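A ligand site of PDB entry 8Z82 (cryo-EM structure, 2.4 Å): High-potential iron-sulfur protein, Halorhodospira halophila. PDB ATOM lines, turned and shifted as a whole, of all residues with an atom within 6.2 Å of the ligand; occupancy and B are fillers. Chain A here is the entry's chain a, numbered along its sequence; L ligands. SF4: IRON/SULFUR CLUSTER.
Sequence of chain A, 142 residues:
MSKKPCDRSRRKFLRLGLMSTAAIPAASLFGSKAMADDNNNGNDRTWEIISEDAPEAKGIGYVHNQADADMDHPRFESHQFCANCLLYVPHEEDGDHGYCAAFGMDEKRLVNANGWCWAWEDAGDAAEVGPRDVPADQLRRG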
ATOM      1  N   ILE A  60     -21.511   5.256  -8.279  1.00  0.00           N
ATOM      2  CA  ILE A  60     -21.623   4.576  -6.990  1.00  0.00           C
ATOM      3  C   ILE A  60     -22.919   4.914  -6.268  1.00  0.00           C
ATOM      4  O   ILE A  60     -23.150   4.403  -5.164  1.00  0.00           O
ATOM      5  CB  ILE A  60     -20.413   4.880  -6.088  1.00  0.00           C
ATOM      6  CG1 ILE A  60     -20.402   6.351  -5.688  1.00  0.00           C
ATOM      7  CG2 ILE A  60     -19.130   4.516  -6.805  1.00  0.00           C
ATOM      8  CD1 ILE A  60     -19.249   6.707  -4.792  1.00  0.00           C
ATOM      9  N   TYR A  62     -23.945   7.971  -5.041  1.00  0.00           N
ATOM     10  CA  TYR A  62     -23.811   8.905  -3.935  1.00  0.00           C
ATOM     11  C   TYR A  62     -25.004   9.844  -3.926  1.00  0.00           C
ATOM     12  O   TYR A  62     -25.240  10.567  -4.893  1.00  0.00           O
ATOM     13  CB  TYR A  62     -22.514   9.702  -4.038  1.00  0.00           C
ATOM     14  CG  TYR A  62     -22.497  10.878  -3.097  1.00  0.00           C
ATOM     15  CD1 TYR A  62     -22.415  10.696  -1.730  1.00  0.00           C
ATOM     16  CD2 TYR A  62     -22.592  12.185  -3.578  1.00  0.00           C
ATOM     17  CE1 TYR A  62     -22.419  11.762  -0.862  1.00  0.00           C
ATOM     18  CE2 TYR A  62     -22.593  13.263  -2.716  1.00  0.00           C
ATOM     19  CZ  TYR A  62     -22.503  13.042  -1.358  1.00  0.00           C
ATOM     20  OH  TYR A  62     -22.501  14.110  -0.496  1.00  0.00           O
ATOM     21  N   PHE A  81     -25.106   5.426   7.007  1.00  0.00           N
ATOM     22  CA  PHE A  81     -24.896   6.810   6.637  1.00  0.00           C
ATOM     23  C   PHE A  81     -23.423   7.010   6.343  1.00  0.00           C
ATOM     24  O   PHE A  81     -22.587   6.145   6.615  1.00  0.00           O
ATOM     25  CB  PHE A  81     -25.340   7.770   7.756  1.00  0.00           C
ATOM     26  CG  PHE A  81     -26.735   7.526   8.249  1.00  0.00           C
ATOM     27  CD1 PHE A  81     -27.813   8.094   7.605  1.00  0.00           C
ATOM     28  CD2 PHE A  81     -26.957   6.729   9.355  1.00  0.00           C
ATOM     29  CE1 PHE A  81     -29.096   7.862   8.054  1.00  0.00           C
ATOM     30  CE2 PHE A  81     -28.233   6.499   9.811  1.00  0.00           C
ATOM     31  CZ  PHE A  81     -29.304   7.070   9.161  1.00  0.00           C
ATOM     32  N   CYS A  82     -23.104   8.179   5.763  1.00  0.00           N
ATOM     33  CA  CYS A  82     -21.710   8.487   5.495  1.00  0.00           C
ATOM     34  C   CYS A  82     -20.885   8.516   6.780  1.00  0.00           C
ATOM     35  O   CYS A  82     -19.759   8.031   6.814  1.00  0.00           O
ATOM     36  CB  CYS A  82     -21.584   9.816   4.755  1.00  0.00           C
ATOM     37  SG  CYS A  82     -21.887   9.711   2.983  1.00  0.00           S
ATOM     38  N   ALA A  83     -21.452   9.089   7.853  1.00  0.00           N
ATOM     39  CA  ALA A  83     -20.740   9.120   9.126  1.00  0.00           C
ATOM     40  C   ALA A  83     -20.461   7.719   9.650  1.00  0.00           C
ATOM     41  O   ALA A  83     -19.438   7.493  10.316  1.00  0.00           O
ATOM     42  CB  ALA A  83     -21.534   9.920  10.156  1.00  0.00           C
ATOM     43  N   CYS A  85     -19.765   5.281   7.736  1.00  0.00           N
ATOM     44  CA  CYS A  85     -18.967   4.610   6.722  1.00  0.00           C
ATOM     45  C   CYS A  85     -17.502   4.522   7.139  1.00  0.00           C
ATOM     46  O   CYS A  85     -16.933   5.469   7.675  1.00  0.00           O
ATOM     47  CB  CYS A  85     -19.087   5.333   5.377  1.00  0.00           C
ATOM     48  SG  CYS A  85     -18.551   4.382   3.950  1.00  0.00           S
ATOM     49  N   LEU A  86     -16.898   3.362   6.884  1.00  0.00           N
ATOM     50  CA  LEU A  86     -15.479   3.169   7.129  1.00  0.00           C
ATOM     51  C   LEU A  86     -14.624   4.107   6.279  1.00  0.00           C
ATOM     52  O   LEU A  86     -13.505   4.446   6.661  1.00  0.00           O
ATOM     53  CB  LEU A  86     -15.116   1.704   6.864  1.00  0.00           C
ATOM     54  CG  LEU A  86     -13.658   1.267   6.753  1.00  0.00           C
ATOM     55  CD1 LEU A  86     -12.950   1.421   8.077  1.00  0.00           C
ATOM     56  CD2 LEU A  86     -13.585  -0.167   6.259  1.00  0.00           C
ATOM     57  N   LEU A  87     -15.137   4.531   5.130  1.00  0.00           N
ATOM     58  CA  LEU A  87     -14.397   5.334   4.174  1.00  0.00           C
ATOM     59  C   LEU A  87     -14.566   6.832   4.399  1.00  0.00           C
ATOM     60  O   LEU A  87     -14.191   7.621   3.526  1.00  0.00           O
ATOM     61  CB  LEU A  87     -14.803   4.979   2.742  1.00  0.00           C
ATOM     62  CG  LEU A  87     -14.631   3.576   2.169  1.00  0.00           C
ATOM     63  CD1 LEU A  87     -15.676   2.616   2.691  1.00  0.00           C
ATOM     64  CD2 LEU A  87     -14.681   3.638   0.660  1.00  0.00           C
ATOM     65  N   TYR A  88     -15.140   7.250   5.518  1.00  0.00           N
ATOM     66  CA  TYR A  88     -15.468   8.643   5.772  1.00  0.00           C
ATOM     67  C   TYR A  88     -14.540   9.228   6.823  1.00  0.00           C
ATOM     68  O   TYR A  88     -14.382   8.651   7.910  1.00  0.00           O
ATOM     69  CB  TYR A  88     -16.918   8.776   6.224  1.00  0.00           C
ATOM     70  CG  TYR A  88     -17.342  10.180   6.595  1.00  0.00           C
ATOM     71  CD1 TYR A  88     -17.583  11.137   5.623  1.00  0.00           C
ATOM     72  CD2 TYR A  88     -17.519  10.534   7.918  1.00  0.00           C
ATOM     73  CE1 TYR A  88     -17.972  12.417   5.959  1.00  0.00           C
ATOM     74  CE2 TYR A  88     -17.909  11.813   8.267  1.00  0.00           C
ATOM     75  CZ  TYR A  88     -18.139  12.743   7.280  1.00  0.00           C
ATOM     76  OH  TYR A  88     -18.525  14.012   7.629  1.00  0.00           O
ATOM     77  N   VAL A  89     -13.921  10.358   6.494  1.00  0.00           N
ATOM     78  CA  VAL A  89     -13.123  11.123   7.460  1.00  0.00           C
ATOM     79  C   VAL A  89     -13.765  12.489   7.585  1.00  0.00           C
ATOM     80  O   VAL A  89     -13.828  13.236   6.599  1.00  0.00           O
ATOM     81  CB  VAL A  89     -11.654  11.222   7.010  1.00  0.00           C
ATOM     82  CG1 VAL A  89     -10.887  12.159   7.930  1.00  0.00           C
ATOM     83  CG2 VAL A  89     -11.022   9.846   6.990  1.00  0.00           C
ATOM     84  N   TYR A  99     -14.244  13.998   4.038  1.00  0.00           N
ATOM     85  CA  TYR A  99     -13.592  13.287   2.944  1.00  0.00           C
ATOM     86  C   TYR A  99     -14.201  11.900   2.745  1.00  0.00           C
ATOM     87  O   TYR A  99     -14.749  11.299   3.673  1.00  0.00           O
ATOM     88  CB  TYR A  99     -12.103  13.163   3.203  1.00  0.00           C
ATOM     89  CG  TYR A  99     -11.343  14.470   3.177  1.00  0.00           C
ATOM     90  CD1 TYR A  99     -11.316  15.309   4.279  1.00  0.00           C
ATOM     91  CD2 TYR A  99     -10.628  14.844   2.048  1.00  0.00           C
ATOM     92  CE1 TYR A  99     -10.618  16.496   4.256  1.00  0.00           C
ATOM     93  CE2 TYR A  99      -9.915  16.016   2.017  1.00  0.00           C
ATOM     94  CZ  TYR A  99      -9.921  16.843   3.110  1.00  0.00           C
ATOM     95  OH  TYR A  99      -9.212  18.025   3.065  1.00  0.00           O
ATOM     96  N   CYS A 100     -14.078  11.391   1.523  1.00  0.00           N
ATOM     97  CA  CYS A 100     -14.541  10.045   1.176  1.00  0.00           C
ATOM     98  C   CYS A 100     -13.403   9.293   0.497  1.00  0.00           C
ATOM     99  O   CYS A 100     -12.836   9.774  -0.482  1.00  0.00           O
ATOM    100  CB  CYS A 100     -15.771  10.099   0.263  1.00  0.00           C
ATOM    101  SG  CYS A 100     -16.230   8.530  -0.468  1.00  0.00           S
ATOM    102  N   ALA A 101     -13.101   8.094   1.015  1.00  0.00           N
ATOM    103  CA  ALA A 101     -11.992   7.312   0.474  1.00  0.00           C
ATOM    104  C   ALA A 101     -12.319   6.759  -0.904  1.00  0.00           C
ATOM    105  O   ALA A 101     -11.416   6.557  -1.718  1.00  0.00           O
ATOM    106  CB  ALA A 101     -11.641   6.184   1.439  1.00  0.00           C
ATOM    107  N   ALA A 102     -13.600   6.514  -1.188  1.00  0.00           N
ATOM    108  CA  ALA A 102     -13.993   6.148  -2.535  1.00  0.00           C
ATOM    109  C   ALA A 102     -13.755   7.266  -3.525  1.00  0.00           C
ATOM    110  O   ALA A 102     -13.715   7.014  -4.733  1.00  0.00           O
ATOM    111  CB  ALA A 102     -15.469   5.729  -2.554  1.00  0.00           C
ATOM    112  N   PHE A 103     -13.603   8.508  -3.049  1.00  0.00           N
ATOM    113  CA  PHE A 103     -13.265   9.635  -3.901  1.00  0.00           C
ATOM    114  C   PHE A 103     -11.808  10.061  -3.733  1.00  0.00           C
ATOM    115  O   PHE A 103     -11.456  11.205  -4.000  1.00  0.00           O
ATOM    116  CB  PHE A 103     -14.191  10.822  -3.622  1.00  0.00           C
ATOM    117  CG  PHE A 103     -15.620  10.555  -3.948  1.00  0.00           C
ATOM    118  CD1 PHE A 103     -15.964   9.843  -5.084  1.00  0.00           C
ATOM    119  CD2 PHE A 103     -16.635  10.992  -3.116  1.00  0.00           C
ATOM    120  CE1 PHE A 103     -17.278   9.586  -5.390  1.00  0.00           C
ATOM    121  CE2 PHE A 103     -17.955  10.733  -3.416  1.00  0.00           C
ATOM    122  CZ  PHE A 103     -18.273  10.031  -4.549  1.00  0.00           C
ATOM    123  N   VAL A 111     -18.234  14.724   1.043  1.00  0.00           N
ATOM    124  CA  VAL A 111     -19.521  14.051   1.092  1.00  0.00           C
ATOM    125  C   VAL A 111     -20.287  14.519   2.320  1.00  0.00           C
ATOM    126  O   VAL A 111     -19.697  14.815   3.372  1.00  0.00           O
ATOM    127  CB  VAL A 111     -19.392  12.514   1.111  1.00  0.00           C
ATOM    128  CG1 VAL A 111     -18.871  12.012  -0.222  1.00  0.00           C
ATOM    129  CG2 VAL A 111     -18.477  12.072   2.246  1.00  0.00           C
ATOM    130  N   ASN A 112     -21.607  14.593   2.185  1.00  0.00           N
ATOM    131  CA  ASN A 112     -22.460  14.949   3.303  1.00  0.00           C
ATOM    132  C   ASN A 112     -22.533  13.797   4.298  1.00  0.00           C
ATOM    133  O   ASN A 112     -22.644  12.630   3.900  1.00  0.00           O
ATOM    134  CB  ASN A 112     -23.870  15.308   2.808  1.00  0.00           C
ATOM    135  CG  ASN A 112     -24.528  16.385   3.636  1.00  0.00           C
ATOM    136  OD1 ASN A 112     -24.968  16.126   4.756  1.00  0.00           O
ATOM    137  ND2 ASN A 112     -24.608  17.583   3.092  1.00  0.00           N
ATOM    138  N   GLY A 115     -25.181  11.312   3.760  1.00  0.00           N
ATOM    139  CA  GLY A 115     -25.217  10.738   2.434  1.00  0.00           C
ATOM    140  C   GLY A 115     -25.118   9.221   2.461  1.00  0.00           C
ATOM    141  O   GLY A 115     -25.137   8.580   3.501  1.00  0.00           O
ATOM    142  N   TRP A 116     -24.999   8.657   1.256  1.00  0.00           N
ATOM    143  CA  TRP A 116     -24.951   7.205   1.107  1.00  0.00           C
ATOM    144  C   TRP A 116     -24.540   6.848  -0.305  1.00  0.00           C
ATOM    145  O   TRP A 116     -24.959   7.512  -1.263  1.00  0.00           O
ATOM    146  CB  TRP A 116     -26.310   6.577   1.418  1.00  0.00           C
ATOM    147  CG  TRP A 116     -26.333   5.085   1.314  1.00  0.00           C
ATOM    148  CD1 TRP A 116     -26.085   4.204   2.313  1.00  0.00           C
ATOM    149  CD2 TRP A 116     -26.615   4.313   0.142  1.00  0.00           C
ATOM    150  NE1 TRP A 116     -26.200   2.922   1.843  1.00  0.00           N
ATOM    151  CE2 TRP A 116     -26.518   2.959   0.513  1.00  0.00           C
ATOM    152  CE3 TRP A 116     -26.942   4.635  -1.176  1.00  0.00           C
ATOM    153  CZ2 TRP A 116     -26.736   1.929  -0.391  1.00  0.00           C
ATOM    154  CZ3 TRP A 116     -27.151   3.598  -2.073  1.00  0.00           C
ATOM    155  CH2 TRP A 116     -27.048   2.265  -1.672  1.00  0.00           C
ATOM    156  N   CYS A 117     -23.727   5.814  -0.436  1.00  0.00           N
ATOM    157  CA  CYS A 117     -23.526   5.145  -1.708  1.00  0.00           C
ATOM    158  C   CYS A 117     -23.359   3.661  -1.415  1.00  0.00           C
ATOM    159  O   CYS A 117     -23.046   3.270  -0.294  1.00  0.00           O
ATOM    160  CB  CYS A 117     -22.332   5.714  -2.478  1.00  0.00           C
ATOM    161  SG  CYS A 117     -20.723   5.283  -1.838  1.00  0.00           S
ATOM    162  N   TRP A 118     -23.600   2.832  -2.433  1.00  0.00           N
ATOM    163  CA  TRP A 118     -23.516   1.394  -2.175  1.00  0.00           C
ATOM    164  C   TRP A 118     -22.099   0.922  -1.936  1.00  0.00           C
ATOM    165  O   TRP A 118     -21.885  -0.280  -1.769  1.00  0.00           O
ATOM    166  CB  TRP A 118     -24.162   0.600  -3.314  1.00  0.00           C
ATOM    167  CG  TRP A 118     -23.694   0.968  -4.673  1.00  0.00           C
ATOM    168  CD1 TRP A 118     -24.351   1.731  -5.577  1.00  0.00           C
ATOM    169  CD2 TRP A 118     -22.471   0.566  -5.303  1.00  0.00           C
ATOM    170  NE1 TRP A 118     -23.620   1.846  -6.730  1.00  0.00           N
ATOM    171  CE2 TRP A 118     -22.465   1.141  -6.582  1.00  0.00           C
ATOM    172  CE3 TRP A 118     -21.389  -0.212  -4.901  1.00  0.00           C
ATOM    173  CZ2 TRP A 118     -21.408   0.947  -7.474  1.00  0.00           C
ATOM    174  CZ3 TRP A 118     -20.340  -0.389  -5.778  1.00  0.00           C
ATOM    175  CH2 TRP A 118     -20.357   0.188  -7.051  1.00  0.00           C
ATOM    176  N   ALA A 119     -21.122   1.828  -1.932  1.00  0.00           N
ATOM    177  CA  ALA A 119     -19.777   1.510  -1.472  1.00  0.00           C
ATOM    178  C   ALA A 119     -19.637   1.610   0.037  1.00  0.00           C
ATOM    179  O   ALA A 119     -18.524   1.459   0.541  1.00  0.00           O
ATOM    180  CB  ALA A 119     -18.766   2.443  -2.132  1.00  0.00           C
ATOM    181  N   TRP A 120     -20.730   1.875   0.741  1.00  0.00           N
ATOM    182  CA  TRP A 120     -20.685   1.997   2.192  1.00  0.00           C
ATOM    183  C   TRP A 120     -20.129   0.728   2.822  1.00  0.00           C
ATOM    184  O   TRP A 120     -20.465  -0.385   2.425  1.00  0.00           O
ATOM    185  CB  TRP A 120     -22.085   2.260   2.755  1.00  0.00           C
ATOM    186  CG  TRP A 120     -22.102   2.441   4.242  1.00  0.00           C
ATOM    187  CD1 TRP A 120     -21.944   3.610   4.919  1.00  0.00           C
ATOM    188  CD2 TRP A 120     -22.289   1.428   5.242  1.00  0.00           C
ATOM    189  NE1 TRP A 120     -22.021   3.391   6.270  1.00  0.00           N
ATOM    190  CE2 TRP A 120     -22.228   2.047   6.494  1.00  0.00           C
ATOM    191  CE3 TRP A 120     -22.483   0.040   5.187  1.00  0.00           C
ATOM    192  CZ2 TRP A 120     -22.366   1.353   7.689  1.00  0.00           C
ATOM    193  CZ3 TRP A 120     -22.631  -0.648   6.375  1.00  0.00           C
ATOM    194  CH2 TRP A 120     -22.573   0.004   7.608  1.00  0.00           C
ATOM    195  N   GLU A 121     -19.268   0.915   3.821  1.00  0.00           N
ATOM    196  CA  GLU A 121     -18.757  -0.187   4.617  1.00  0.00           C
ATOM    197  C   GLU A 121     -18.794   0.213   6.076  1.00  0.00           C
ATOM    198  O   GLU A 121     -18.697   1.388   6.403  1.00  0.00           O
ATOM    199  CB  GLU A 121     -17.346  -0.582   4.187  1.00  0.00           C
ATOM    200  CG  GLU A 121     -17.322  -1.404   2.917  1.00  0.00           C
ATOM    201  CD  GLU A 121     -17.815  -2.813   3.132  1.00  0.00           C
ATOM    202  OE1 GLU A 121     -18.250  -3.145   4.255  1.00  0.00           O
ATOM    203  OE2 GLU A 121     -17.768  -3.611   2.185  1.00  0.00           O
HETATM  204 FE1  SF4 L   1     -20.197   7.835   2.405  1.00  0.00          FE
HETATM  205 FE2  SF4 L   1     -18.682   5.570   2.424  1.00  0.00          FE
HETATM  206 FE3  SF4 L   1     -18.196   7.514   0.564  1.00  0.00          FE
HETATM  207 FE4  SF4 L   1     -20.469   5.998   0.400  1.00  0.00          FE
HETATM  208  S1  SF4 L   1     -18.320   5.270   0.197  1.00  0.00           S
HETATM  209  S2  SF4 L   1     -20.309   8.256   0.159  1.00  0.00           S
HETATM  210  S3  SF4 L   1     -20.951   5.696   2.608  1.00  0.00           S
HETATM  211  S4  SF4 L   1     -17.969   7.693   2.821  1.00  0.00           S
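SG of Cys 85 binds FE2 of the ligand.
SG of Cys 117 is bound to FE4 of the ligand (2.4 Å).
The side-chain sulfur (SG) of Cys 100 binds an iron atom (FE3) of the ligand, 2.4 Å away.
SG of Cys 82 binds FE1 of the ligand, at 2.6 Å.
SG of Cys 85 lies close to N of Glu 121.
The backbone NH (N) of Ala 119 lies close to the side-chain sulfur (SG) of Cys 117.
The backbone NH of Phe 103 sits close to the side-chain sulfur of Cys 100 (3.7 Å).
O of Gly 115 is in hydrogen-bond range of N of Cys 82 (3.1 Å).
SG of Cys 82 lies close to O of Asn 112 (3.2 Å).
NE1 of Trp 120 sits at hydrogen-bond distance from O of Phe 81 (2.8 Å).
The side-chain hydroxyl (OH) of Tyr 62 is in hydrogen-bond range of the backbone NH (N) of Asn 112, at 2.9 Å.
The backbone carbonyl oxygen (O) of Leu 87 lies within hydrogen-bond range of the backbone NH (N) of Ala 101, 2.8 Å away.
CD1 of Tyr 62 touches S2 of the ligand, at 3.7 Å.
Leu 87 touches the ligand.
CB of Tyr 88 touches S4 of the ligand, 3.7 Å away.
CB of Ala 102 touches S1 of the ligand, 3.99 Å away.
CB of Ala 119 touches S1 of the ligand (3.7 Å).
CD1 of Trp 120 touches S3 of the ligand, at 3.3 Å.
Hydrophobic or aromatic side chains within 4 Å of the ligand: Tyr 62, Leu 87, Tyr 88, Ala 102, Ala 119 and Trp 120.
Of the 24 residues printed, 10 come within 4 Å of the ligand.
The nearest printed residue that does not touch the ligand is Val 111 (4.04 Å).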
